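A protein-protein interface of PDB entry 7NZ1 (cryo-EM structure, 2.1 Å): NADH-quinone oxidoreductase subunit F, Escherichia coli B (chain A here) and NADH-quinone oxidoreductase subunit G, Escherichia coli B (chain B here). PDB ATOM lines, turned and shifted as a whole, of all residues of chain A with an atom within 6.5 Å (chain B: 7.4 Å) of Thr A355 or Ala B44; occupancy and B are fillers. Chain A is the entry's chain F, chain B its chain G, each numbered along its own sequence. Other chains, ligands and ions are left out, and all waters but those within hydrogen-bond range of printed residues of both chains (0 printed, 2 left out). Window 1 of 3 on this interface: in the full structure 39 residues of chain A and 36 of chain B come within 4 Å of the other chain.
Trp A353 touches Val B42. Trp A353 touches Tyr B155 (CZ3 to CD2, 3.6 Å). N of Thr A355 touches O of Ala B44, at 3.6 Å. Thr A355 touches Leu B95 (CG2 to CD2, 3.8 Å). Arg B46 touches Pro A356 (CG to CD, 3.7 Å). CZ3 of Trp B94 touches CB of Pro A356, at 3.6 Å. Asp A359 touches Trp B94. Gly A360 touches Trp B94. Phe A397 touches Gly B43. NH1 of Arg B46 touches CD1 of Phe A397 (3.6 Å).
The guanidinium group of Arg A358 sits at hydrogen-bond distance from the backbone carbonyl oxygen of Gly A352 (2.9 Å). The guanidinium group (NH2) of Arg A358 sits at hydrogen-bond distance from the side-chain hydroxyl (OG1) of Thr A355 (3.1 Å). N of Phe B33 sits close to SG of Cys B45, at 3.6 Å. O of Gly B43 lies within hydrogen-bond range of NH1 of Arg B46. SD of Met B68 sits at hydrogen-bond distance from N of Gly B43. SG of Cys B45 sits close to N of Gln B47, at 3.4 Å.
Of the 24 printed residues of chain B, 10 touch a printed residue of chain A. Hydrophobic or aromatic side chains of chain B within 4 Å of the printed part of chain A: Val B42, Ala B44, Trp B94, Leu B95, Ala B153 and Tyr B155. Of the 12 printed residues of chain A, 10 touch a printed residue of chain B. Hydrophobic or aromatic side chains of chain A within 4 Å of the printed part of chain B: Trp A353, Pro A356 and Phe A397. Among the printed residues, no Asp or Glu carboxylate lies within 4 Å of a Lys or Arg side-chain nitrogen of the other chain.
Printed residues of chain B within 4 Å of Thr A355: Ala B44, Cys B45 and Leu B95. Of chain A, only Trp A353, Cys A354 and Thr A355 come within 4 Å of Ala B44. Printed residues of chain B within 4 Å of Thr A396: Arg B46. Of the printed residues of chain B, Phe A397 touches Val B42 (3.3 Å), Gly B43 (3.3 Å) and Arg B46 (3.6 Å). Ser B90 touches none of the printed residues of chain A.
O of Gly A352 is in hydrogen-bond range of OH of Tyr B155 (3.0 Å). The side-chain hydroxyl (OG1) of Thr A355 is in hydrogen-bond range of the backbone carbonyl oxygen (O) of Cys B45 (3.0 Å). The guanidinium group of Arg A358 lies within hydrogen-bond range of the backbone carbonyl oxygen of Ile B152 (3.4 Å). The backbone carbonyl oxygen (O) of Thr A396 lies within hydrogen-bond range of the guanidinium group (NH2) of Arg B46 (3.3 Å).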
ATOM      1  N   GLY A 352     -13.064   3.208  23.720  1.00  0.00           N
ATOM      2  CA  GLY A 352     -14.434   2.878  23.401  1.00  0.00           C
ATOM      3  C   GLY A 352     -15.481   3.846  23.906  1.00  0.00           C
ATOM      4  O   GLY A 352     -16.672   3.591  23.705  1.00  0.00           O
ATOM      5  N   TRP A 353     -15.079   4.934  24.569  1.00  0.00           N
ATOM      6  CA  TRP A 353     -16.036   5.870  25.154  1.00  0.00           C
ATOM      7  C   TRP A 353     -16.797   6.665  24.095  1.00  0.00           C
ATOM      8  O   TRP A 353     -18.029   6.724  24.125  1.00  0.00           O
ATOM      9  CB  TRP A 353     -15.313   6.802  26.120  1.00  0.00           C
ATOM     10  CG  TRP A 353     -16.152   7.826  26.779  1.00  0.00           C
ATOM     11  CD1 TRP A 353     -16.175   9.163  26.517  1.00  0.00           C
ATOM     12  CD2 TRP A 353     -17.097   7.605  27.827  1.00  0.00           C
ATOM     13  NE1 TRP A 353     -17.069   9.790  27.345  1.00  0.00           N
ATOM     14  CE2 TRP A 353     -17.649   8.856  28.159  1.00  0.00           C
ATOM     15  CE3 TRP A 353     -17.532   6.471  28.516  1.00  0.00           C
ATOM     16  CZ2 TRP A 353     -18.617   9.002  29.146  1.00  0.00           C
ATOM     17  CZ3 TRP A 353     -18.490   6.624  29.502  1.00  0.00           C
ATOM     18  CH2 TRP A 353     -19.019   7.877  29.805  1.00  0.00           C
ATOM     19  N   CYS A 354     -16.090   7.295  23.162  1.00  0.00           N
ATOM     20  CA  CYS A 354     -16.726   8.240  22.255  1.00  0.00           C
ATOM     21  C   CYS A 354     -16.827   7.688  20.838  1.00  0.00           C
ATOM     22  O   CYS A 354     -15.908   7.024  20.350  1.00  0.00           O
ATOM     23  CB  CYS A 354     -16.018   9.603  22.282  1.00  0.00           C
ATOM     24  SG  CYS A 354     -14.458   9.750  21.429  1.00  0.00           S
ATOM     25  N   THR A 355     -17.977   7.958  20.212  1.00  0.00           N
ATOM     26  CA  THR A 355     -18.338   7.468  18.876  1.00  0.00           C
ATOM     27  C   THR A 355     -17.324   7.714  17.747  1.00  0.00           C
ATOM     28  O   THR A 355     -17.044   6.754  17.013  1.00  0.00           O
ATOM     29  CB  THR A 355     -19.718   8.040  18.497  1.00  0.00           C
ATOM     30  OG1 THR A 355     -20.647   7.818  19.561  1.00  0.00           O
ATOM     31  CG2 THR A 355     -20.250   7.385  17.238  1.00  0.00           C
ATOM     32  N   PRO A 356     -16.751   8.923  17.524  1.00  0.00           N
ATOM     33  CA  PRO A 356     -15.883   9.082  16.338  1.00  0.00           C
ATOM     34  C   PRO A 356     -14.545   8.374  16.443  1.00  0.00           C
ATOM     35  O   PRO A 356     -13.907   8.135  15.415  1.00  0.00           O
ATOM     36  CB  PRO A 356     -15.675  10.602  16.250  1.00  0.00           C
ATOM     37  CG  PRO A 356     -16.657  11.193  17.167  1.00  0.00           C
ATOM     38  CD  PRO A 356     -16.788  10.209  18.249  1.00  0.00           C
ATOM     39  N   CYS A 357     -14.133   7.983  17.639  1.00  0.00           N
ATOM     40  CA  CYS A 357     -12.956   7.151  17.820  1.00  0.00           C
ATOM     41  C   CYS A 357     -13.309   5.674  17.748  1.00  0.00           C
ATOM     42  O   CYS A 357     -12.660   4.916  17.019  1.00  0.00           O
ATOM     43  CB  CYS A 357     -12.293   7.469  19.160  1.00  0.00           C
ATOM     44  SG  CYS A 357     -10.684   6.695  19.414  1.00  0.00           S
ATOM     45  N   ARG A 358     -14.339   5.274  18.500  1.00  0.00           N
ATOM     46  CA  ARG A 358     -14.769   3.881  18.576  1.00  0.00           C
ATOM     47  C   ARG A 358     -15.247   3.349  17.227  1.00  0.00           C
ATOM     48  O   ARG A 358     -14.962   2.203  16.871  1.00  0.00           O
ATOM     49  CB  ARG A 358     -15.873   3.749  19.626  1.00  0.00           C
ATOM     50  CG  ARG A 358     -16.402   2.348  19.818  1.00  0.00           C
ATOM     51  CD  ARG A 358     -17.657   2.222  20.700  1.00  0.00           C
ATOM     52  NE  ARG A 358     -18.791   3.025  20.256  1.00  0.00           N
ATOM     53  CZ  ARG A 358     -19.113   4.217  20.740  1.00  0.00           C
ATOM     54  NH1 ARG A 358     -18.416   4.777  21.710  1.00  0.00           N
ATOM     55  NH2 ARG A 358     -20.159   4.861  20.238  1.00  0.00           N
ATOM     56  N   ASP A 359     -15.985   4.154  16.469  1.00  0.00           N
ATOM     57  CA  ASP A 359     -16.552   3.685  15.210  1.00  0.00           C
ATOM     58  C   ASP A 359     -15.918   4.300  13.971  1.00  0.00           C
ATOM     59  O   ASP A 359     -15.943   3.668  12.914  1.00  0.00           O
ATOM     60  CB  ASP A 359     -18.063   3.934  15.178  1.00  0.00           C
ATOM     61  CG  ASP A 359     -18.777   3.294  16.348  1.00  0.00           C
ATOM     62  OD1 ASP A 359     -19.038   2.076  16.300  1.00  0.00           O
ATOM     63  OD2 ASP A 359     -19.080   4.008  17.322  1.00  0.00           O
ATOM     64  N   GLY A 360     -15.382   5.519  14.065  1.00  0.00           N
ATOM     65  CA  GLY A 360     -14.750   6.136  12.906  1.00  0.00           C
ATOM     66  C   GLY A 360     -13.447   5.468  12.497  1.00  0.00           C
ATOM     67  O   GLY A 360     -13.237   5.177  11.318  1.00  0.00           O
ATOM     68  N   LEU A 361     -12.550   5.241  13.463  1.00  0.00           N
ATOM     69  CA  LEU A 361     -11.259   4.609  13.178  1.00  0.00           C
ATOM     70  C   LEU A 361     -11.315   3.189  12.596  1.00  0.00           C
ATOM     71  O   LEU A 361     -10.457   2.894  11.745  1.00  0.00           O
ATOM     72  CB  LEU A 361     -10.364   4.626  14.428  1.00  0.00           C
ATOM     73  CG  LEU A 361      -9.705   5.917  14.898  1.00  0.00           C
ATOM     74  CD1 LEU A 361      -8.861   5.645  16.126  1.00  0.00           C
ATOM     75  CD2 LEU A 361      -8.858   6.518  13.790  1.00  0.00           C
ATOM     76  N   THR A 396     -13.707  14.812  19.430  1.00  0.00           N
ATOM     77  CA  THR A 396     -13.705  13.593  20.221  1.00  0.00           C
ATOM     78  C   THR A 396     -13.456  13.930  21.685  1.00  0.00           C
ATOM     79  O   THR A 396     -13.135  15.066  22.038  1.00  0.00           O
ATOM     80  CB  THR A 396     -12.655  12.606  19.698  1.00  0.00           C
ATOM     81  OG1 THR A 396     -11.361  13.220  19.719  1.00  0.00           O
ATOM     82  CG2 THR A 396     -12.989  12.199  18.292  1.00  0.00           C
ATOM     83  N   PHE A 397     -13.618  12.918  22.540  1.00  0.00           N
ATOM     84  CA  PHE A 397     -13.596  13.152  23.980  1.00  0.00           C
ATOM     85  C   PHE A 397     -12.186  13.416  24.500  1.00  0.00           C
ATOM     86  O   PHE A 397     -12.019  14.202  25.435  1.00  0.00           O
ATOM     87  CB  PHE A 397     -14.226  11.975  24.723  1.00  0.00           C
ATOM     88  CG  PHE A 397     -14.563  12.275  26.154  1.00  0.00           C
ATOM     89  CD1 PHE A 397     -15.698  13.002  26.472  1.00  0.00           C
ATOM     90  CD2 PHE A 397     -13.741  11.834  27.185  1.00  0.00           C
ATOM     91  CE1 PHE A 397     -16.011  13.283  27.786  1.00  0.00           C
ATOM     92  CE2 PHE A 397     -14.049  12.113  28.505  1.00  0.00           C
ATOM     93  CZ  PHE A 397     -15.188  12.836  28.804  1.00  0.00           C
ATOM     94  N   PHE B  33     -27.974  11.307  22.218  1.00  0.00           N
ATOM     95  CA  PHE B  33     -28.160   9.958  22.739  1.00  0.00           C
ATOM     96  C   PHE B  33     -27.746   9.801  24.192  1.00  0.00           C
ATOM     97  O   PHE B  33     -28.532   9.293  24.995  1.00  0.00           O
ATOM     98  CB  PHE B  33     -27.396   8.944  21.883  1.00  0.00           C
ATOM     99  CG  PHE B  33     -27.914   8.822  20.497  1.00  0.00           C
ATOM    100  CD1 PHE B  33     -29.142   8.225  20.250  1.00  0.00           C
ATOM    101  CD2 PHE B  33     -27.170   9.296  19.431  1.00  0.00           C
ATOM    102  CE1 PHE B  33     -29.614   8.106  18.960  1.00  0.00           C
ATOM    103  CE2 PHE B  33     -27.636   9.182  18.146  1.00  0.00           C
ATOM    104  CZ  PHE B  33     -28.857   8.591  17.911  1.00  0.00           C
ATOM    105  N   CYS B  34     -26.533  10.224  24.561  1.00  0.00           N
ATOM    106  CA  CYS B  34     -25.977   9.815  25.846  1.00  0.00           C
ATOM    107  C   CYS B  34     -26.459  10.680  27.002  1.00  0.00           C
ATOM    108  O   CYS B  34     -26.370  10.251  28.154  1.00  0.00           O
ATOM    109  CB  CYS B  34     -24.442   9.801  25.794  1.00  0.00           C
ATOM    110  SG  CYS B  34     -23.590  11.376  25.777  1.00  0.00           S
ATOM    111  N   TRP B  35     -26.957  11.875  26.725  1.00  0.00           N
ATOM    112  CA  TRP B  35     -27.506  12.729  27.765  1.00  0.00           C
ATOM    113  C   TRP B  35     -28.893  12.246  28.177  1.00  0.00           C
ATOM    114  O   TRP B  35     -29.665  11.756  27.353  1.00  0.00           O
ATOM    115  CB  TRP B  35     -27.569  14.173  27.276  1.00  0.00           C
ATOM    116  CG  TRP B  35     -28.258  15.116  28.203  1.00  0.00           C
ATOM    117  CD1 TRP B  35     -27.720  15.743  29.283  1.00  0.00           C
ATOM    118  CD2 TRP B  35     -29.621  15.533  28.134  1.00  0.00           C
ATOM    119  NE1 TRP B  35     -28.660  16.533  29.889  1.00  0.00           N
ATOM    120  CE2 TRP B  35     -29.838  16.425  29.199  1.00  0.00           C
ATOM    121  CE3 TRP B  35     -30.679  15.242  27.272  1.00  0.00           C
ATOM    122  CZ2 TRP B  35     -31.071  17.026  29.428  1.00  0.00           C
ATOM    123  CZ3 TRP B  35     -31.901  15.843  27.495  1.00  0.00           C
ATOM    124  CH2 TRP B  35     -32.086  16.725  28.567  1.00  0.00           C
ATOM    125  N   SER B  41     -24.908  14.853  32.196  1.00  0.00           N
ATOM    126  CA  SER B  41     -24.117  14.918  30.973  1.00  0.00           C
ATOM    127  C   SER B  41     -22.770  14.238  31.163  1.00  0.00           C
ATOM    128  O   SER B  41     -22.088  14.482  32.161  1.00  0.00           O
ATOM    129  CB  SER B  41     -23.894  16.367  30.542  1.00  0.00           C
ATOM    130  OG  SER B  41     -25.101  17.079  30.400  1.00  0.00           O
ATOM    131  N   VAL B  42     -22.378  13.400  30.201  1.00  0.00           N
ATOM    132  CA  VAL B  42     -21.051  12.793  30.251  1.00  0.00           C
ATOM    133  C   VAL B  42     -20.236  13.086  28.999  1.00  0.00           C
ATOM    134  O   VAL B  42     -19.003  13.115  29.051  1.00  0.00           O
ATOM    135  CB  VAL B  42     -21.141  11.277  30.491  1.00  0.00           C
ATOM    136  CG1 VAL B  42     -21.429  11.022  31.944  1.00  0.00           C
ATOM    137  CG2 VAL B  42     -22.195  10.644  29.594  1.00  0.00           C
ATOM    138  N   GLY B  43     -20.899  13.291  27.869  1.00  0.00           N
ATOM    139  CA  GLY B  43     -20.191  13.677  26.669  1.00  0.00           C
ATOM    140  C   GLY B  43     -19.715  12.552  25.785  1.00  0.00           C
ATOM    141  O   GLY B  43     -18.694  12.706  25.111  1.00  0.00           O
ATOM    142  N   ALA B  44     -20.405  11.415  25.780  1.00  0.00           N
ATOM    143  CA  ALA B  44     -19.886  10.227  25.121  1.00  0.00           C
ATOM    144  C   ALA B  44     -20.278  10.146  23.649  1.00  0.00           C
ATOM    145  O   ALA B  44     -19.410   9.957  22.796  1.00  0.00           O
ATOM    146  CB  ALA B  44     -20.361   8.969  25.857  1.00  0.00           C
ATOM    147  N   CYS B  45     -21.564  10.305  23.329  1.00  0.00           N
ATOM    148  CA  CYS B  45     -22.044   9.977  21.991  1.00  0.00           C
ATOM    149  C   CYS B  45     -21.612  10.979  20.922  1.00  0.00           C
ATOM    150  O   CYS B  45     -21.597  10.618  19.744  1.00  0.00           O
ATOM    151  CB  CYS B  45     -23.565   9.870  21.985  1.00  0.00           C
ATOM    152  SG  CYS B  45     -24.383  11.435  22.206  1.00  0.00           S
ATOM    153  N   ARG B  46     -21.295  12.216  21.321  1.00  0.00           N
ATOM    154  CA  ARG B  46     -20.889  13.336  20.453  1.00  0.00           C
ATOM    155  C   ARG B  46     -21.965  13.721  19.432  1.00  0.00           C
ATOM    156  O   ARG B  46     -21.659  14.292  18.389  1.00  0.00           O
ATOM    157  CB  ARG B  46     -19.551  13.081  19.738  1.00  0.00           C
ATOM    158  CG  ARG B  46     -18.442  12.491  20.591  1.00  0.00           C
ATOM    159  CD  ARG B  46     -18.129  13.262  21.852  1.00  0.00           C
ATOM    160  NE  ARG B  46     -17.293  14.430  21.616  1.00  0.00           N
ATOM    161  CZ  ARG B  46     -16.872  15.243  22.573  1.00  0.00           C
ATOM    162  NH1 ARG B  46     -17.188  15.038  23.840  1.00  0.00           N
ATOM    163  NH2 ARG B  46     -16.135  16.300  22.251  1.00  0.00           N
ATOM    164  N   GLN B  47     -23.233  13.442  19.724  1.00  0.00           N
ATOM    165  CA  GLN B  47     -24.300  13.706  18.768  1.00  0.00           C
ATOM    166  C   GLN B  47     -24.856  15.123  18.900  1.00  0.00           C
ATOM    167  O   GLN B  47     -25.347  15.681  17.917  1.00  0.00           O
ATOM    168  CB  GLN B  47     -25.417  12.665  18.958  1.00  0.00           C
ATOM    169  CG  GLN B  47     -26.628  12.758  18.037  1.00  0.00           C
ATOM    170  CD  GLN B  47     -26.238  12.641  16.578  1.00  0.00           C
ATOM    171  OE1 GLN B  47     -26.031  11.546  16.082  1.00  0.00           O
ATOM    172  NE2 GLN B  47     -26.116  13.770  15.896  1.00  0.00           N
ATOM    173  N   MET B  65     -19.861  20.365  22.354  1.00  0.00           N
ATOM    174  CA  MET B  65     -21.011  19.526  22.659  1.00  0.00           C
ATOM    175  C   MET B  65     -21.923  20.289  23.603  1.00  0.00           C
ATOM    176  O   MET B  65     -21.479  20.759  24.652  1.00  0.00           O
ATOM    177  CB  MET B  65     -20.604  18.191  23.277  1.00  0.00           C
ATOM    178  CG  MET B  65     -19.542  17.504  22.497  1.00  0.00           C
ATOM    179  SD  MET B  65     -20.214  16.858  20.971  1.00  0.00           S
ATOM    180  CE  MET B  65     -18.961  17.426  19.829  1.00  0.00           C
ATOM    181  N   CYS B  67     -24.470  19.396  25.452  1.00  0.00           N
ATOM    182  CA  CYS B  67     -24.694  18.808  26.765  1.00  0.00           C
ATOM    183  C   CYS B  67     -23.537  19.098  27.718  1.00  0.00           C
ATOM    184  O   CYS B  67     -23.749  19.193  28.929  1.00  0.00           O
ATOM    185  CB  CYS B  67     -24.943  17.304  26.626  1.00  0.00           C
ATOM    186  SG  CYS B  67     -23.489  16.304  26.290  1.00  0.00           S
ATOM    187  N   MET B  68     -22.328  19.289  27.198  1.00  0.00           N
ATOM    188  CA  MET B  68     -21.159  19.562  28.021  1.00  0.00           C
ATOM    189  C   MET B  68     -20.794  21.041  28.095  1.00  0.00           C
ATOM    190  O   MET B  68     -19.798  21.382  28.733  1.00  0.00           O
ATOM    191  CB  MET B  68     -19.961  18.765  27.504  1.00  0.00           C
ATOM    192  CG  MET B  68     -20.113  17.266  27.648  1.00  0.00           C
ATOM    193  SD  MET B  68     -20.474  16.709  29.326  1.00  0.00           S
ATOM    194  CE  MET B  68     -18.829  16.634  30.021  1.00  0.00           C
ATOM    195  N   SER B  90     -22.673  12.615  10.415  1.00  0.00           N
ATOM    196  CA  SER B  90     -21.596  11.626  10.454  1.00  0.00           C
ATOM    197  C   SER B  90     -21.659  10.743  11.697  1.00  0.00           C
ATOM    198  O   SER B  90     -21.298   9.563  11.633  1.00  0.00           O
ATOM    199  CB  SER B  90     -20.242  12.323  10.377  1.00  0.00           C
ATOM    200  OG  SER B  90     -20.089  12.990   9.146  1.00  0.00           O
ATOM    201  N   VAL B  91     -22.048  11.316  12.844  1.00  0.00           N
ATOM    202  CA  VAL B  91     -22.184  10.547  14.084  1.00  0.00           C
ATOM    203  C   VAL B  91     -23.253   9.468  13.929  1.00  0.00           C
ATOM    204  O   VAL B  91     -23.049   8.315  14.328  1.00  0.00           O
ATOM    205  CB  VAL B  91     -22.470  11.492  15.270  1.00  0.00           C
ATOM    206  CG1 VAL B  91     -22.838  10.715  16.531  1.00  0.00           C
ATOM    207  CG2 VAL B  91     -21.270  12.379  15.548  1.00  0.00           C
ATOM    208  N   VAL B  92     -24.385   9.817  13.305  1.00  0.00           N
ATOM    209  CA  VAL B  92     -25.425   8.840  12.972  1.00  0.00           C
ATOM    210  C   VAL B  92     -24.900   7.811  11.969  1.00  0.00           C
ATOM    211  O   VAL B  92     -25.175   6.611  12.098  1.00  0.00           O
ATOM    212  CB  VAL B  92     -26.692   9.572  12.471  1.00  0.00           C
ATOM    213  CG1 VAL B  92     -27.525   8.735  11.515  1.00  0.00           C
ATOM    214  CG2 VAL B  92     -27.554   9.948  13.642  1.00  0.00           C
ATOM    215  N   GLU B  93     -24.095   8.261  10.996  1.00  0.00           N
ATOM    216  CA  GLU B  93     -23.512   7.357  10.000  1.00  0.00           C
ATOM    217  C   GLU B  93     -22.559   6.352  10.641  1.00  0.00           C
ATOM    218  O   GLU B  93     -22.578   5.166  10.296  1.00  0.00           O
ATOM    219  CB  GLU B  93     -22.778   8.154   8.919  1.00  0.00           C
ATOM    220  CG  GLU B  93     -22.104   7.278   7.870  1.00  0.00           C
ATOM    221  CD  GLU B  93     -21.904   7.964   6.542  1.00  0.00           C
ATOM    222  OE1 GLU B  93     -21.237   9.018   6.513  1.00  0.00           O
ATOM    223  OE2 GLU B  93     -22.401   7.444   5.526  1.00  0.00           O
ATOM    224  N   TRP B  94     -21.752   6.805  11.604  1.00  0.00           N
ATOM    225  CA  TRP B  94     -20.848   5.907  12.316  1.00  0.00           C
ATOM    226  C   TRP B  94     -21.600   4.912  13.194  1.00  0.00           C
ATOM    227  O   TRP B  94     -21.156   3.771  13.346  1.00  0.00           O
ATOM    228  CB  TRP B  94     -19.875   6.718  13.166  1.00  0.00           C
ATOM    229  CG  TRP B  94     -18.827   7.419  12.368  1.00  0.00           C
ATOM    230  CD1 TRP B  94     -18.181   6.942  11.269  1.00  0.00           C
ATOM    231  CD2 TRP B  94     -18.314   8.734  12.595  1.00  0.00           C
ATOM    232  NE1 TRP B  94     -17.289   7.871  10.803  1.00  0.00           N
ATOM    233  CE2 TRP B  94     -17.353   8.983  11.597  1.00  0.00           C
ATOM    234  CE3 TRP B  94     -18.570   9.724  13.546  1.00  0.00           C
ATOM    235  CZ2 TRP B  94     -16.647  10.178  11.525  1.00  0.00           C
ATOM    236  CZ3 TRP B  94     -17.874  10.909  13.470  1.00  0.00           C
ATOM    237  CH2 TRP B  94     -16.920  11.127  12.469  1.00  0.00           C
ATOM    238  N   LEU B  95     -22.747   5.309  13.750  1.00  0.00           N
ATOM    239  CA  LEU B  95     -23.548   4.372  14.529  1.00  0.00           C
ATOM    240  C   LEU B  95     -24.280   3.382  13.638  1.00  0.00           C
ATOM    241  O   LEU B  95     -24.552   2.257  14.062  1.00  0.00           O
ATOM    242  CB  LEU B  95     -24.545   5.134  15.398  1.00  0.00           C
ATOM    243  CG  LEU B  95     -23.923   5.953  16.522  1.00  0.00           C
ATOM    244  CD1 LEU B  95     -24.982   6.767  17.225  1.00  0.00           C
ATOM    245  CD2 LEU B  95     -23.212   5.043  17.495  1.00  0.00           C
ATOM    246  N   ILE B 152     -25.703   1.047  20.720  1.00  0.00           N
ATOM    247  CA  ILE B 152     -24.956   2.144  20.120  1.00  0.00           C
ATOM    248  C   ILE B 152     -23.899   2.696  21.065  1.00  0.00           C
ATOM    249  O   ILE B 152     -23.298   3.731  20.762  1.00  0.00           O
ATOM    250  CB  ILE B 152     -25.887   3.268  19.636  1.00  0.00           C
ATOM    251  CG1 ILE B 152     -26.767   3.758  20.783  1.00  0.00           C
ATOM    252  CG2 ILE B 152     -26.719   2.789  18.474  1.00  0.00           C
ATOM    253  CD1 ILE B 152     -27.351   5.101  20.574  1.00  0.00           C
ATOM    254  N   ALA B 153     -23.691   2.040  22.222  1.00  0.00           N
ATOM    255  CA  ALA B 153     -22.678   2.390  23.234  1.00  0.00           C
ATOM    256  C   ALA B 153     -22.857   3.813  23.766  1.00  0.00           C
ATOM    257  O   ALA B 153     -21.915   4.597  23.837  1.00  0.00           O
ATOM    258  CB  ALA B 153     -21.253   2.165  22.712  1.00  0.00           C
ATOM    259  N   CYS B 154     -24.096   4.153  24.116  1.00  0.00           N
ATOM    260  CA  CYS B 154     -24.401   5.456  24.687  1.00  0.00           C
ATOM    261  C   CYS B 154     -24.166   5.528  26.190  1.00  0.00           C
ATOM    262  O   CYS B 154     -24.203   6.630  26.742  1.00  0.00           O
ATOM    263  CB  CYS B 154     -25.852   5.836  24.386  1.00  0.00           C
ATOM    264  SG  CYS B 154     -27.084   4.921  25.331  1.00  0.00           S
ATOM    265  N   TYR B 155     -23.969   4.383  26.851  1.00  0.00           N
ATOM    266  CA  TYR B 155     -23.668   4.205  28.275  1.00  0.00           C
ATOM    267  C   TYR B 155     -24.802   4.638  29.194  1.00  0.00           C
ATOM    268  O   TYR B 155     -24.574   4.776  30.393  1.00  0.00           O
ATOM    269  CB  TYR B 155     -22.373   4.921  28.717  1.00  0.00           C
ATOM    270  CG  TYR B 155     -21.100   4.358  28.120  1.00  0.00           C
ATOM    271  CD1 TYR B 155     -20.750   4.629  26.802  1.00  0.00           C
ATOM    272  CD2 TYR B 155     -20.248   3.557  28.874  1.00  0.00           C
ATOM    273  CE1 TYR B 155     -19.599   4.116  26.244  1.00  0.00           C
ATOM    274  CE2 TYR B 155     -19.090   3.034  28.322  1.00  0.00           C
ATOM    275  CZ  TYR B 155     -18.774   3.317  27.005  1.00  0.00           C
ATOM    276  OH  TYR B 155     -17.629   2.815  26.443  1.00  0.00           O
ATOM    277  N   ARG B 159     -25.039   3.968  33.523  1.00  0.00           N
ATOM    278  CA  ARG B 159     -25.178   5.179  34.327  1.00  0.00           C
ATOM    279  C   ARG B 159     -26.493   5.192  35.099  1.00  0.00           C
ATOM    280  O   ARG B 159     -26.555   5.727  36.205  1.00  0.00           O
ATOM    281  CB  ARG B 159     -25.025   6.421  33.453  1.00  0.00           C
ATOM    282  CG  ARG B 159     -23.608   6.554  32.940  1.00  0.00           C
ATOM    283  CD  ARG B 159     -23.244   7.895  32.344  1.00  0.00           C
ATOM    284  NE  ARG B 159     -24.271   8.567  31.556  1.00  0.00           N
ATOM    285  CZ  ARG B 159     -24.963   9.623  31.960  1.00  0.00           C
ATOM    286  NH1 ARG B 159     -24.773  10.158  33.155  1.00  0.00           N
ATOM    287  NH2 ARG B 159     -25.853  10.167  31.139  1.00  0.00           N
